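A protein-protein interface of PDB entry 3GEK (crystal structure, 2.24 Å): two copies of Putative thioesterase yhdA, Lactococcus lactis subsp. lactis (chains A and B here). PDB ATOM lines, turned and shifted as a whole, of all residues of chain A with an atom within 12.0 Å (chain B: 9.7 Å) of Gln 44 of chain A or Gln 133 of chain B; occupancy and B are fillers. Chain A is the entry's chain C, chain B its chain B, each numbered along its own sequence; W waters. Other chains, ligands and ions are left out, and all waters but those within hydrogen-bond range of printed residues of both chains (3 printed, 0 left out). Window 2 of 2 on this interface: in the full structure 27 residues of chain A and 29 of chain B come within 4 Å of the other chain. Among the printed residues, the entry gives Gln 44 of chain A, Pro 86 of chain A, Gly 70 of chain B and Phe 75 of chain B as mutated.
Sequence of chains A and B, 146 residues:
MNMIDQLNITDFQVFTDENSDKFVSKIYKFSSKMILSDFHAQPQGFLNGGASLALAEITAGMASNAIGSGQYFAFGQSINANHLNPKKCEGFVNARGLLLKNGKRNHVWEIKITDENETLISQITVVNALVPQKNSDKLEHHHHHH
OD1 of Asn 48 of chain A is in hydrogen-bond range of N of Gly 50 of chain A (2.9 Å).
O of Gly 70 of chain B lies within hydrogen-bond range of NE2 of Gln 133 of chain B, at 3.2 Å.
O of His 40 of chain A lies within hydrogen-bond range of N of Asn 48 of chain A (2.7 Å).
NE2 of Gln 42 of chain A lies within hydrogen-bond range of OE1 of Gln 44 of chain A, at 2.9 Å.
The backbone NH (N) of Gln 133 of chain B is in hydrogen-bond range of the backbone carbonyl oxygen (O) of Gln 71 of chain B (3.0 Å).
N of Phe 73 of chain B lies within hydrogen-bond range of O of Val 131 of chain B (3.0 Å).
Among the printed residues, pairs that only touch across the chains: Asp 38 of chain A with Asn 2 of chain B (3.2 Å), Asn 48 of chain A with Ile 4 of chain B (3.4 Å), Gln 44 of chain A with Phe 73 of chain B (3.5 Å), Phe 39 of chain A with Asn 2 of chain B (3.5 Å), Gln 44 of chain A with Gln 133 of chain B (3.7 Å), Pro 86 of chain A with Phe 75 of chain B (3.8 Å) and Ala 41 of chain A with Ile 4 of chain B (3.9 Å).
No residue of chain B comes within 4 Å of Pro 43 of chain A.
Of chain B, only Phe 73 and Gln 133 come within 4 Å of Gln 44 of chain A.
Printed residues of chain B within 4 Å of Asn 48 of chain A: Ile 4.
Gly 50 of chain A touches none of the printed residues of chain B.
Printed residues of chain A within 4 Å of Ile 4 of chain B: Ala 41 (3.9 Å) and Asn 48 (3.4 Å).
No residue of chain A comes within 4 Å of Ala 74 of chain B.
Leu 130 of chain B touches none of the printed residues of chain A.
No residue of chain A comes within 4 Å of Val 131 of chain B.
Gln 133 of chain B touches just one residue of chain A: Gln 44.
The nearest residue of chain B that does not touch Gln 44 of chain A is Ala 74 of chain B (4.8 Å).
Hydrophobic or aromatic side chains of chain B within 4 Å of the printed part of chain A: Ile 4, Phe 73 and Phe 75.
Hydrophobic or aromatic side chains of chain A within 4 Å of the printed part of chain B: Phe 39 and Pro 86.
No position is printed for both chains.
Water W3 bridges O of Asp 38 of chain A (2.5 Å) and ND2 of Asn 2 of chain B (3.1 Å).
Water W1 lies within hydrogen-bond range of the backbone carbonyl oxygen of Ala 41 of chain A (2.7 Å), the backbone carbonyl oxygen of Phe 39 of chain A (2.8 Å), the backbone NH of Ile 4 of chain B (3.5 Å) and the side-chain amide nitrogen of Asn 48 of chain A (3.5 Å).
Water W2 lies within hydrogen-bond range of OE1 of Gln 44 of chain A (2.7 Å), O of Ala 74 of chain B (2.7 Å) and ND2 of Asn 65 of chain B (3.2 Å).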
ATOM      1  N   SER A  37       4.858 -28.584 -12.981  1.00  0.00           N
ATOM      2  CA  SER A  37       3.825 -27.875 -13.727  1.00  0.00           C
ATOM      3  C   SER A  37       3.992 -26.398 -13.389  1.00  0.00           C
ATOM      4  O   SER A  37       4.931 -26.033 -12.684  1.00  0.00           O
ATOM      5  CB  SER A  37       2.428 -28.372 -13.341  1.00  0.00           C
ATOM      6  OG  SER A  37       2.130 -28.067 -11.987  1.00  0.00           O
ATOM      7  N   ASP A  38       3.091 -25.549 -13.868  1.00  0.00           N
ATOM      8  CA  ASP A  38       3.176 -24.120 -13.545  1.00  0.00           C
ATOM      9  C   ASP A  38       2.870 -23.815 -12.070  1.00  0.00           C
ATOM     10  O   ASP A  38       3.048 -22.680 -11.622  1.00  0.00           O
ATOM     11  CB  ASP A  38       2.308 -23.279 -14.483  1.00  0.00           C
ATOM     12  CG  ASP A  38       0.936 -23.852 -14.668  1.00  0.00           C
ATOM     13  OD1 ASP A  38       0.209 -23.969 -13.655  1.00  0.00           O
ATOM     14  OD2 ASP A  38       0.585 -24.184 -15.827  1.00  0.00           O
ATOM     15  N   PHE A  39       2.427 -24.830 -11.325  1.00  0.00           N
ATOM     16  CA  PHE A  39       2.279 -24.719  -9.872  1.00  0.00           C
ATOM     17  C   PHE A  39       3.625 -24.342  -9.267  1.00  0.00           C
ATOM     18  O   PHE A  39       3.693 -23.543  -8.334  1.00  0.00           O
ATOM     19  CB  PHE A  39       1.765 -26.039  -9.268  1.00  0.00           C
ATOM     20  CG  PHE A  39       1.754 -26.063  -7.753  1.00  0.00           C
ATOM     21  CD1 PHE A  39       0.656 -25.583  -7.039  1.00  0.00           C
ATOM     22  CD2 PHE A  39       2.837 -26.577  -7.040  1.00  0.00           C
ATOM     23  CE1 PHE A  39       0.642 -25.606  -5.640  1.00  0.00           C
ATOM     24  CE2 PHE A  39       2.831 -26.603  -5.638  1.00  0.00           C
ATOM     25  CZ  PHE A  39       1.732 -26.116  -4.940  1.00  0.00           C
ATOM     26  N   HIS A  40       4.686 -24.913  -9.839  1.00  0.00           N
ATOM     27  CA  HIS A  40       6.058 -24.776  -9.341  1.00  0.00           C
ATOM     28  C   HIS A  40       6.766 -23.512  -9.826  1.00  0.00           C
ATOM     29  O   HIS A  40       7.875 -23.223  -9.380  1.00  0.00           O
ATOM     30  CB  HIS A  40       6.887 -25.996  -9.763  1.00  0.00           C
ATOM     31  CG  HIS A  40       6.242 -27.307  -9.443  1.00  0.00           C
ATOM     32  ND1 HIS A  40       6.611 -28.072  -8.358  1.00  0.00           N
ATOM     33  CD2 HIS A  40       5.240 -27.979 -10.055  1.00  0.00           C
ATOM     34  CE1 HIS A  40       5.869 -29.163  -8.321  1.00  0.00           C
ATOM     35  NE2 HIS A  40       5.031 -29.133  -9.341  1.00  0.00           N
ATOM     36  N   ALA A  41       6.133 -22.775 -10.736  1.00  0.00           N
ATOM     37  CA  ALA A  41       6.785 -21.652 -11.422  1.00  0.00           C
ATOM     38  C   ALA A  41       6.805 -20.346 -10.625  1.00  0.00           C
ATOM     39  O   ALA A  41       5.875 -20.055  -9.867  1.00  0.00           O
ATOM     40  CB  ALA A  41       6.141 -21.422 -12.792  1.00  0.00           C
ATOM     41  N   GLN A  42       7.882 -19.578 -10.796  1.00  0.00           N
ATOM     42  CA  GLN A  42       7.932 -18.179 -10.359  1.00  0.00           C
ATOM     43  C   GLN A  42       7.700 -17.264 -11.588  1.00  0.00           C
ATOM     44  O   GLN A  42       7.703 -17.757 -12.720  1.00  0.00           O
ATOM     45  CB  GLN A  42       9.236 -17.867  -9.593  1.00  0.00           C
ATOM     46  CG  GLN A  42      10.537 -18.248 -10.292  1.00  0.00           C
ATOM     47  CD  GLN A  42      10.947 -17.252 -11.369  1.00  0.00           C
ATOM     48  OE1 GLN A  42      10.673 -17.457 -12.554  1.00  0.00           O
ATOM     49  NE2 GLN A  42      11.594 -16.162 -10.958  1.00  0.00           N
ATOM     50  N   PRO A  43       7.483 -15.945 -11.372  1.00  0.00           N
ATOM     51  CA  PRO A  43       6.973 -15.047 -12.432  1.00  0.00           C
ATOM     52  C   PRO A  43       7.710 -15.013 -13.783  1.00  0.00           C
ATOM     53  O   PRO A  43       7.106 -14.625 -14.785  1.00  0.00           O
ATOM     54  CB  PRO A  43       7.000 -13.668 -11.764  1.00  0.00           C
ATOM     55  CG  PRO A  43       6.835 -13.971 -10.295  1.00  0.00           C
ATOM     56  CD  PRO A  43       7.661 -15.216 -10.097  1.00  0.00           C
ATOM     57  N   GLN A  44       8.985 -15.396 -13.814  1.00  0.00           N
ATOM     58  CA  GLN A  44       9.769 -15.353 -15.056  1.00  0.00           C
ATOM     59  C   GLN A  44       9.772 -16.686 -15.808  1.00  0.00           C
ATOM     60  O   GLN A  44      10.410 -16.811 -16.855  1.00  0.00           O
ATOM     61  CB  GLN A  44      11.206 -14.880 -14.789  1.00  0.00           C
ATOM     62  CG  GLN A  44      11.351 -13.366 -14.598  1.00  0.00           C
ATOM     63  CD  GLN A  44      10.864 -12.890 -13.237  1.00  0.00           C
ATOM     64  OE1 GLN A  44      11.002 -13.590 -12.234  1.00  0.00           O
ATOM     65  NE2 GLN A  44      10.291 -11.694 -13.199  1.00  0.00           N
ATOM     66  N   GLY A  45       9.054 -17.672 -15.272  1.00  0.00           N
ATOM     67  CA  GLY A  45       8.927 -18.974 -15.926  1.00  0.00           C
ATOM     68  C   GLY A  45       9.940 -20.008 -15.465  1.00  0.00           C
ATOM     69  O   GLY A  45      10.045 -21.088 -16.052  1.00  0.00           O
ATOM     70  N   PHE A  46      10.688 -19.681 -14.416  1.00  0.00           N
ATOM     71  CA  PHE A  46      11.650 -20.620 -13.849  1.00  0.00           C
ATOM     72  C   PHE A  46      11.040 -21.392 -12.692  1.00  0.00           C
ATOM     73  O   PHE A  46      10.030 -20.979 -12.117  1.00  0.00           O
ATOM     74  CB  PHE A  46      12.920 -19.898 -13.375  1.00  0.00           C
ATOM     75  CG  PHE A  46      13.695 -19.236 -14.482  1.00  0.00           C
ATOM     76  CD1 PHE A  46      14.446 -19.996 -15.379  1.00  0.00           C
ATOM     77  CD2 PHE A  46      13.685 -17.852 -14.621  1.00  0.00           C
ATOM     78  CE1 PHE A  46      15.167 -19.387 -16.407  1.00  0.00           C
ATOM     79  CE2 PHE A  46      14.400 -17.233 -15.645  1.00  0.00           C
ATOM     80  CZ  PHE A  46      15.142 -18.005 -16.540  1.00  0.00           C
ATOM     81  N   LEU A  47      11.657 -22.521 -12.360  1.00  0.00           N
ATOM     82  CA  LEU A  47      11.287 -23.275 -11.178  1.00  0.00           C
ATOM     83  C   LEU A  47      11.485 -22.389  -9.955  1.00  0.00           C
ATOM     84  O   LEU A  47      12.555 -21.801  -9.765  1.00  0.00           O
ATOM     85  CB  LEU A  47      12.118 -24.562 -11.074  1.00  0.00           C
ATOM     86  CG  LEU A  47      12.190 -25.348  -9.757  1.00  0.00           C
ATOM     87  CD1 LEU A  47      10.825 -25.879  -9.305  1.00  0.00           C
ATOM     88  CD2 LEU A  47      13.200 -26.482  -9.870  1.00  0.00           C
ATOM     89  N   ASN A  48      10.437 -22.289  -9.144  1.00  0.00           N
ATOM     90  CA  ASN A  48      10.470 -21.531  -7.901  1.00  0.00           C
ATOM     91  C   ASN A  48      11.422 -22.199  -6.917  1.00  0.00           C
ATOM     92  O   ASN A  48      11.242 -23.367  -6.568  1.00  0.00           O
ATOM     93  CB  ASN A  48       9.061 -21.462  -7.304  1.00  0.00           C
ATOM     94  CG  ASN A  48       8.901 -20.354  -6.276  1.00  0.00           C
ATOM     95  OD1 ASN A  48       9.766 -20.121  -5.435  1.00  0.00           O
ATOM     96  ND2 ASN A  48       7.770 -19.676  -6.333  1.00  0.00           N
ATOM     97  N   GLY A  49      12.434 -21.456  -6.475  1.00  0.00           N
ATOM     98  CA  GLY A  49      13.361 -21.936  -5.450  1.00  0.00           C
ATOM     99  C   GLY A  49      12.663 -22.449  -4.201  1.00  0.00           C
ATOM    100  O   GLY A  49      13.129 -23.404  -3.573  1.00  0.00           O
ATOM    101  N   GLY A  50      11.537 -21.824  -3.855  1.00  0.00           N
ATOM    102  CA  GLY A  50      10.716 -22.236  -2.718  1.00  0.00           C
ATOM    103  C   GLY A  50      10.155 -23.644  -2.836  1.00  0.00           C
ATOM    104  O   GLY A  50       9.978 -24.333  -1.828  1.00  0.00           O
ATOM    105  N   PRO A  86      19.584 -21.882 -12.669  1.00  0.00           N
ATOM    106  CA  PRO A  86      18.148 -21.751 -12.897  1.00  0.00           C
ATOM    107  C   PRO A  86      17.626 -22.903 -13.744  1.00  0.00           C
ATOM    108  O   PRO A  86      18.348 -23.421 -14.600  1.00  0.00           O
ATOM    109  CB  PRO A  86      18.031 -20.428 -13.664  1.00  0.00           C
ATOM    110  CG  PRO A  86      19.365 -20.246 -14.310  1.00  0.00           C
ATOM    111  CD  PRO A  86      20.355 -20.822 -13.345  1.00  0.00           C
ATOM    112  N   LYS A  87      16.390 -23.315 -13.489  1.00  0.00           N
ATOM    113  CA  LYS A  87      15.735 -24.286 -14.349  1.00  0.00           C
ATOM    114  C   LYS A  87      14.405 -23.741 -14.844  1.00  0.00           C
ATOM    115  O   LYS A  87      13.646 -23.149 -14.076  1.00  0.00           O
ATOM    116  CB  LYS A  87      15.518 -25.617 -13.626  1.00  0.00           C
ATOM    117  CG  LYS A  87      15.231 -26.765 -14.592  1.00  0.00           C
ATOM    118  CD  LYS A  87      14.523 -27.918 -13.913  1.00  0.00           C
ATOM    119  CE  LYS A  87      14.398 -29.112 -14.844  1.00  0.00           C
ATOM    120  NZ  LYS A  87      13.529 -28.842 -16.033  1.00  0.00           N
ATOM    121  N   LYS A  88      14.136 -23.941 -16.132  1.00  0.00           N
ATOM    122  CA  LYS A  88      12.832 -23.644 -16.705  1.00  0.00           C
ATOM    123  C   LYS A  88      11.801 -24.576 -16.083  1.00  0.00           C
ATOM    124  O   LYS A  88      12.060 -25.771 -15.908  1.00  0.00           O
ATOM    125  CB  LYS A  88      12.856 -23.815 -18.226  1.00  0.00           C
ATOM    126  CG  LYS A  88      13.253 -22.561 -18.997  1.00  0.00           C
ATOM    127  CD  LYS A  88      12.055 -21.640 -19.227  1.00  0.00           C
ATOM    128  CE  LYS A  88      12.412 -20.467 -20.137  1.00  0.00           C
ATOM    129  NZ  LYS A  88      11.191 -19.803 -20.698  1.00  0.00           N
ATOM    130  N   CYS A  89      10.639 -24.030 -15.744  1.00  0.00           N
ATOM    131  CA  CYS A  89       9.623 -24.805 -15.045  1.00  0.00           C
ATOM    132  C   CYS A  89       8.889 -25.757 -15.992  1.00  0.00           C
ATOM    133  O   CYS A  89       7.780 -25.478 -16.446  1.00  0.00           O
ATOM    134  CB  CYS A  89       8.647 -23.892 -14.308  1.00  0.00           C
ATOM    135  SG  CYS A  89       7.693 -24.772 -13.065  1.00  0.00           S
ATOM    136  N   GLU A  90       9.540 -26.882 -16.268  1.00  0.00           N
ATOM    137  CA  GLU A  90       9.052 -27.912 -17.179  1.00  0.00           C
ATOM    138  C   GLU A  90       9.765 -29.224 -16.857  1.00  0.00           C
ATOM    139  O   GLU A  90      10.840 -29.216 -16.257  1.00  0.00           O
ATOM    140  CB  GLU A  90       9.308 -27.513 -18.642  1.00  0.00           C
ATOM    141  CG  GLU A  90      10.716 -26.972 -18.911  1.00  0.00           C
ATOM    142  CD  GLU A  90      11.075 -26.921 -20.388  1.00  0.00           C
ATOM    143  OE1 GLU A  90      10.198 -26.592 -21.218  1.00  0.00           O
ATOM    144  OE2 GLU A  90      12.251 -27.209 -20.716  1.00  0.00           O
ATOM    145  N   ASN B   2      -1.031 -21.194  -8.827  1.00  0.00           N
ATOM    146  CA  ASN B   2       0.257 -21.809  -8.558  1.00  0.00           C
ATOM    147  C   ASN B   2       0.541 -21.886  -7.051  1.00  0.00           C
ATOM    148  O   ASN B   2      -0.336 -21.586  -6.231  1.00  0.00           O
ATOM    149  CB  ASN B   2       1.382 -21.096  -9.327  1.00  0.00           C
ATOM    150  CG  ASN B   2       1.497 -19.610  -8.995  1.00  0.00           C
ATOM    151  OD1 ASN B   2       1.124 -19.151  -7.906  1.00  0.00           O
ATOM    152  ND2 ASN B   2       2.038 -18.851  -9.943  1.00  0.00           N
ATOM    153  N   ILE B   4       2.620 -19.972  -5.299  1.00  0.00           N
ATOM    154  CA  ILE B   4       2.649 -18.611  -4.755  1.00  0.00           C
ATOM    155  C   ILE B   4       1.248 -18.129  -4.350  1.00  0.00           C
ATOM    156  O   ILE B   4       1.065 -17.643  -3.237  1.00  0.00           O
ATOM    157  CB  ILE B   4       3.337 -17.600  -5.715  1.00  0.00           C
ATOM    158  CG1 ILE B   4       4.817 -17.962  -5.905  1.00  0.00           C
ATOM    159  CG2 ILE B   4       3.192 -16.155  -5.188  1.00  0.00           C
ATOM    160  CD1 ILE B   4       5.490 -17.273  -7.090  1.00  0.00           C
ATOM    161  N   GLY B  61      12.115 -12.209  -2.596  1.00  0.00           N
ATOM    162  CA  GLY B  61      12.055 -11.940  -4.043  1.00  0.00           C
ATOM    163  C   GLY B  61      11.058 -10.853  -4.422  1.00  0.00           C
ATOM    164  O   GLY B  61      11.340 -10.018  -5.285  1.00  0.00           O
ATOM    165  N   MET B  62       9.906 -10.864  -3.780  1.00  0.00           N
ATOM    166  CA  MET B  62       8.886  -9.823  -3.963  1.00  0.00           C
ATOM    167  C   MET B  62       9.381  -8.455  -3.515  1.00  0.00           C
ATOM    168  O   MET B  62       9.076  -7.442  -4.147  1.00  0.00           O
ATOM    169  CB  MET B  62       7.621 -10.157  -3.170  1.00  0.00           C
ATOM    170  CG  MET B  62       6.714 -11.203  -3.795  1.00  0.00           C
ATOM    171  SD  MET B  62       5.216 -11.583  -2.597  1.00  0.00           S
ATOM    172  CE  MET B  62       4.155  -9.973  -2.923  1.00  0.00           C
ATOM    173  N   SER B  64      12.634  -7.458  -3.183  1.00  0.00           N
ATOM    174  CA  SER B  64      13.710  -7.016  -4.065  1.00  0.00           C
ATOM    175  C   SER B  64      13.166  -6.461  -5.377  1.00  0.00           C
ATOM    176  O   SER B  64      13.653  -5.444  -5.873  1.00  0.00           O
ATOM    177  CB  SER B  64      14.700  -8.145  -4.346  1.00  0.00           C
ATOM    178  OG  SER B  64      15.522  -8.398  -3.223  1.00  0.00           O
ATOM    179  N   ASN B  65      12.153  -7.128  -5.931  1.00  0.00           N
ATOM    180  CA  ASN B  65      11.528  -6.696  -7.184  1.00  0.00           C
ATOM    181  C   ASN B  65      10.858  -5.331  -7.075  1.00  0.00           C
ATOM    182  O   ASN B  65      10.848  -4.560  -8.038  1.00  0.00           O
ATOM    183  CB  ASN B  65      10.526  -7.743  -7.681  1.00  0.00           C
ATOM    184  CG  ASN B  65      11.204  -8.971  -8.254  1.00  0.00           C
ATOM    185  OD1 ASN B  65      12.398  -8.952  -8.551  1.00  0.00           O
ATOM    186  ND2 ASN B  65      10.447 -10.047  -8.407  1.00  0.00           N
ATOM    187  N   ALA B  66      10.306  -5.047  -5.897  1.00  0.00           N
ATOM    188  CA  ALA B  66       9.673  -3.767  -5.601  1.00  0.00           C
ATOM    189  C   ALA B  66      10.699  -2.638  -5.501  1.00  0.00           C
ATOM    190  O   ALA B  66      10.394  -1.487  -5.819  1.00  0.00           O
ATOM    191  CB  ALA B  66       8.864  -3.866  -4.319  1.00  0.00           C
ATOM    192  N   GLY B  68      13.624  -2.842  -7.197  1.00  0.00           N
ATOM    193  CA  GLY B  68      14.222  -2.788  -8.531  1.00  0.00           C
ATOM    194  C   GLY B  68      13.537  -1.910  -9.560  1.00  0.00           C
ATOM    195  O   GLY B  68      14.163  -1.498 -10.539  1.00  0.00           O
ATOM    196  N   SER B  69      12.251  -1.638  -9.337  1.00  0.00           N
ATOM    197  CA  SER B  69      11.427  -0.823 -10.232  1.00  0.00           C
ATOM    198  C   SER B  69      11.531  -1.232 -11.710  1.00  0.00           C
ATOM    199  O   SER B  69      11.598  -0.384 -12.599  1.00  0.00           O
ATOM    200  CB  SER B  69      11.713   0.671 -10.022  1.00  0.00           C
ATOM    201  OG  SER B  69      11.518   1.017  -8.658  1.00  0.00           O
ATOM    202  N   GLY B  70      11.540  -2.540 -11.953  1.00  0.00           N
ATOM    203  CA  GLY B  70      11.536  -3.087 -13.309  1.00  0.00           C
ATOM    204  C   GLY B  70      12.899  -3.243 -13.963  1.00  0.00           C
ATOM    205  O   GLY B  70      13.004  -3.815 -15.053  1.00  0.00           O
ATOM    206  N   GLN B  71      13.944  -2.746 -13.302  1.00  0.00           N
ATOM    207  CA  GLN B  71      15.295  -2.761 -13.871  1.00  0.00           C
ATOM    208  C   GLN B  71      15.922  -4.149 -13.819  1.00  0.00           C
ATOM    209  O   GLN B  71      16.787  -4.485 -14.634  1.00  0.00           O
ATOM    210  CB  GLN B  71      16.194  -1.733 -13.176  1.00  0.00           C
ATOM    211  CG  GLN B  71      15.658  -0.291 -13.198  1.00  0.00           C
ATOM    212  CD  GLN B  71      15.447   0.275 -14.605  1.00  0.00           C
ATOM    213  OE1 GLN B  71      16.096  -0.142 -15.568  1.00  0.00           O
ATOM    214  NE2 GLN B  71      14.538   1.240 -14.720  1.00  0.00           N
ATOM    215  N   TYR B  72      15.471  -4.948 -12.854  1.00  0.00           N
ATOM    216  CA  TYR B  72      15.942  -6.314 -12.674  1.00  0.00           C
ATOM    217  C   TYR B  72      14.858  -7.150 -12.003  1.00  0.00           C
ATOM    218  O   TYR B  72      13.914  -6.599 -11.433  1.00  0.00           O
ATOM    219  CB  TYR B  72      17.235  -6.337 -11.839  1.00  0.00           C
ATOM    220  CG  TYR B  72      17.134  -5.645 -10.489  1.00  0.00           C
ATOM    221  CD1 TYR B  72      16.514  -6.273  -9.403  1.00  0.00           C
ATOM    222  CD2 TYR B  72      17.671  -4.368 -10.292  1.00  0.00           C
ATOM    223  CE1 TYR B  72      16.416  -5.646  -8.163  1.00  0.00           C
ATOM    224  CE2 TYR B  72      17.586  -3.731  -9.048  1.00  0.00           C
ATOM    225  CZ  TYR B  72      16.958  -4.383  -7.988  1.00  0.00           C
ATOM    226  OH  TYR B  72      16.857  -3.774  -6.758  1.00  0.00           O
ATOM    227  N   PHE B  73      14.989  -8.474 -12.084  1.00  0.00           N
ATOM    228  CA  PHE B  73      14.173  -9.382 -11.276  1.00  0.00           C
ATOM    229  C   PHE B  73      15.050 -10.183 -10.319  1.00  0.00           C
ATOM    230  O   PHE B  73      16.180 -10.538 -10.656  1.00  0.00           O
ATOM    231  CB  PHE B  73      13.293 -10.302 -12.143  1.00  0.00           C
ATOM    232  CG  PHE B  73      14.062 -11.312 -12.969  1.00  0.00           C
ATOM    233  CD1 PHE B  73      14.384 -12.568 -12.448  1.00  0.00           C
ATOM    234  CD2 PHE B  73      14.432 -11.021 -14.283  1.00  0.00           C
ATOM    235  CE1 PHE B  73      15.083 -13.508 -13.212  1.00  0.00           C
ATOM    236  CE2 PHE B  73      15.131 -11.953 -15.057  1.00  0.00           C
ATOM    237  CZ  PHE B  73      15.458 -13.199 -14.519  1.00  0.00           C
ATOM    238  N   ALA B  74      14.530 -10.450  -9.124  1.00  0.00           N
ATOM    239  CA  ALA B  74      15.277 -11.188  -8.109  1.00  0.00           C
ATOM    240  C   ALA B  74      15.176 -12.689  -8.333  1.00  0.00           C
ATOM    241  O   ALA B  74      14.099 -13.214  -8.629  1.00  0.00           O
ATOM    242  CB  ALA B  74      14.797 -10.824  -6.709  1.00  0.00           C
ATOM    243  N   PHE B  75      16.314 -13.363  -8.210  1.00  0.00           N
ATOM    244  CA  PHE B  75      16.372 -14.808  -8.271  1.00  0.00           C
ATOM    245  C   PHE B  75      17.057 -15.295  -6.998  1.00  0.00           C
ATOM    246  O   PHE B  75      18.183 -14.887  -6.693  1.00  0.00           O
ATOM    247  CB  PHE B  75      17.122 -15.270  -9.530  1.00  0.00           C
ATOM    248  CG  PHE B  75      17.228 -16.775  -9.663  1.00  0.00           C
ATOM    249  CD1 PHE B  75      16.205 -17.511 -10.269  1.00  0.00           C
ATOM    250  CD2 PHE B  75      18.349 -17.456  -9.186  1.00  0.00           C
ATOM    251  CE1 PHE B  75      16.296 -18.906 -10.390  1.00  0.00           C
ATOM    252  CE2 PHE B  75      18.449 -18.844  -9.301  1.00  0.00           C
ATOM    253  CZ  PHE B  75      17.422 -19.570  -9.906  1.00  0.00           C
ATOM    254  N   GLY B  76      16.365 -16.150  -6.251  1.00  0.00           N
ATOM    255  CA  GLY B  76      16.894 -16.702  -5.003  1.00  0.00           C
ATOM    256  C   GLY B  76      18.187 -17.465  -5.226  1.00  0.00           C
ATOM    257  O   GLY B  76      18.238 -18.362  -6.063  1.00  0.00           O
ATOM    258  N   ALA B 129      20.031 -12.926  -6.119  1.00  0.00           N
ATOM    259  CA  ALA B 129      20.770 -12.402  -7.262  1.00  0.00           C
ATOM    260  C   ALA B 129      19.862 -11.431  -8.000  1.00  0.00           C
ATOM    261  O   ALA B 129      18.658 -11.663  -8.129  1.00  0.00           O
ATOM    262  CB  ALA B 129      21.222 -13.520  -8.185  1.00  0.00           C
ATOM    263  N   LEU B 130      20.445 -10.330  -8.457  1.00  0.00           N
ATOM    264  CA  LEU B 130      19.712  -9.286  -9.151  1.00  0.00           C
ATOM    265  C   LEU B 130      20.060  -9.346 -10.636  1.00  0.00           C
ATOM    266  O   LEU B 130      21.120  -8.874 -11.049  1.00  0.00           O
ATOM    267  CB  LEU B 130      20.077  -7.920  -8.559  1.00  0.00           C
ATOM    268  CG  LEU B 130      19.384  -7.359  -7.304  1.00  0.00           C
ATOM    269  CD1 LEU B 130      18.787  -8.408  -6.360  1.00  0.00           C
ATOM    270  CD2 LEU B 130      20.323  -6.421  -6.554  1.00  0.00           C
ATOM    271  N   VAL B 131      19.180  -9.950 -11.430  1.00  0.00           N
ATOM    272  CA  VAL B 131      19.448 -10.143 -12.858  1.00  0.00           C
ATOM    273  C   VAL B 131      18.713  -9.118 -13.732  1.00  0.00           C
ATOM    274  O   VAL B 131      17.486  -9.008 -13.663  1.00  0.00           O
ATOM    275  CB  VAL B 131      19.265 -11.636 -13.331  1.00  0.00           C
ATOM    276  CG1 VAL B 131      18.307 -12.406 -12.439  1.00  0.00           C
ATOM    277  CG2 VAL B 131      18.867 -11.734 -14.806  1.00  0.00           C
ATOM    278  N   PRO B 132      19.476  -8.364 -14.553  1.00  0.00           N
ATOM    279  CA  PRO B 132      18.975  -7.325 -15.454  1.00  0.00           C
ATOM    280  C   PRO B 132      17.791  -7.796 -16.293  1.00  0.00           C
ATOM    281  O   PRO B 132      17.769  -8.943 -16.754  1.00  0.00           O
ATOM    282  CB  PRO B 132      20.181  -7.039 -16.353  1.00  0.00           C
ATOM    283  CG  PRO B 132      21.347  -7.321 -15.494  1.00  0.00           C
ATOM    284  CD  PRO B 132      20.943  -8.500 -14.652  1.00  0.00           C
ATOM    285  N   GLN B 133      16.816  -6.911 -16.475  1.00  0.00           N
ATOM    286  CA  GLN B 133      15.586  -7.236 -17.185  1.00  0.00           C
ATOM    287  C   GLN B 133      15.378  -6.290 -18.364  1.00  0.00           C
ATOM    288  O   GLN B 133      15.991  -6.453 -19.418  1.00  0.00           O
ATOM    289  CB  GLN B 133      14.400  -7.146 -16.225  1.00  0.00           C
ATOM    290  CG  GLN B 133      13.139  -7.858 -16.692  1.00  0.00           C
ATOM    291  CD  GLN B 133      12.057  -7.881 -15.628  1.00  0.00           C
ATOM    292  OE1 GLN B 133      11.486  -8.931 -15.332  1.00  0.00           O
ATOM    293  NE2 GLN B 133      11.767  -6.720 -15.047  1.00  0.00           N
HETATM  294  O   HOH W   1       4.887 -21.137  -7.635  1.00  0.00           O
HETATM  295  O   HOH W   2      11.670 -12.693  -9.772  1.00  0.00           O
HETATM  296  O   HOH W   3       2.348 -20.458 -12.572  1.00  0.00           O
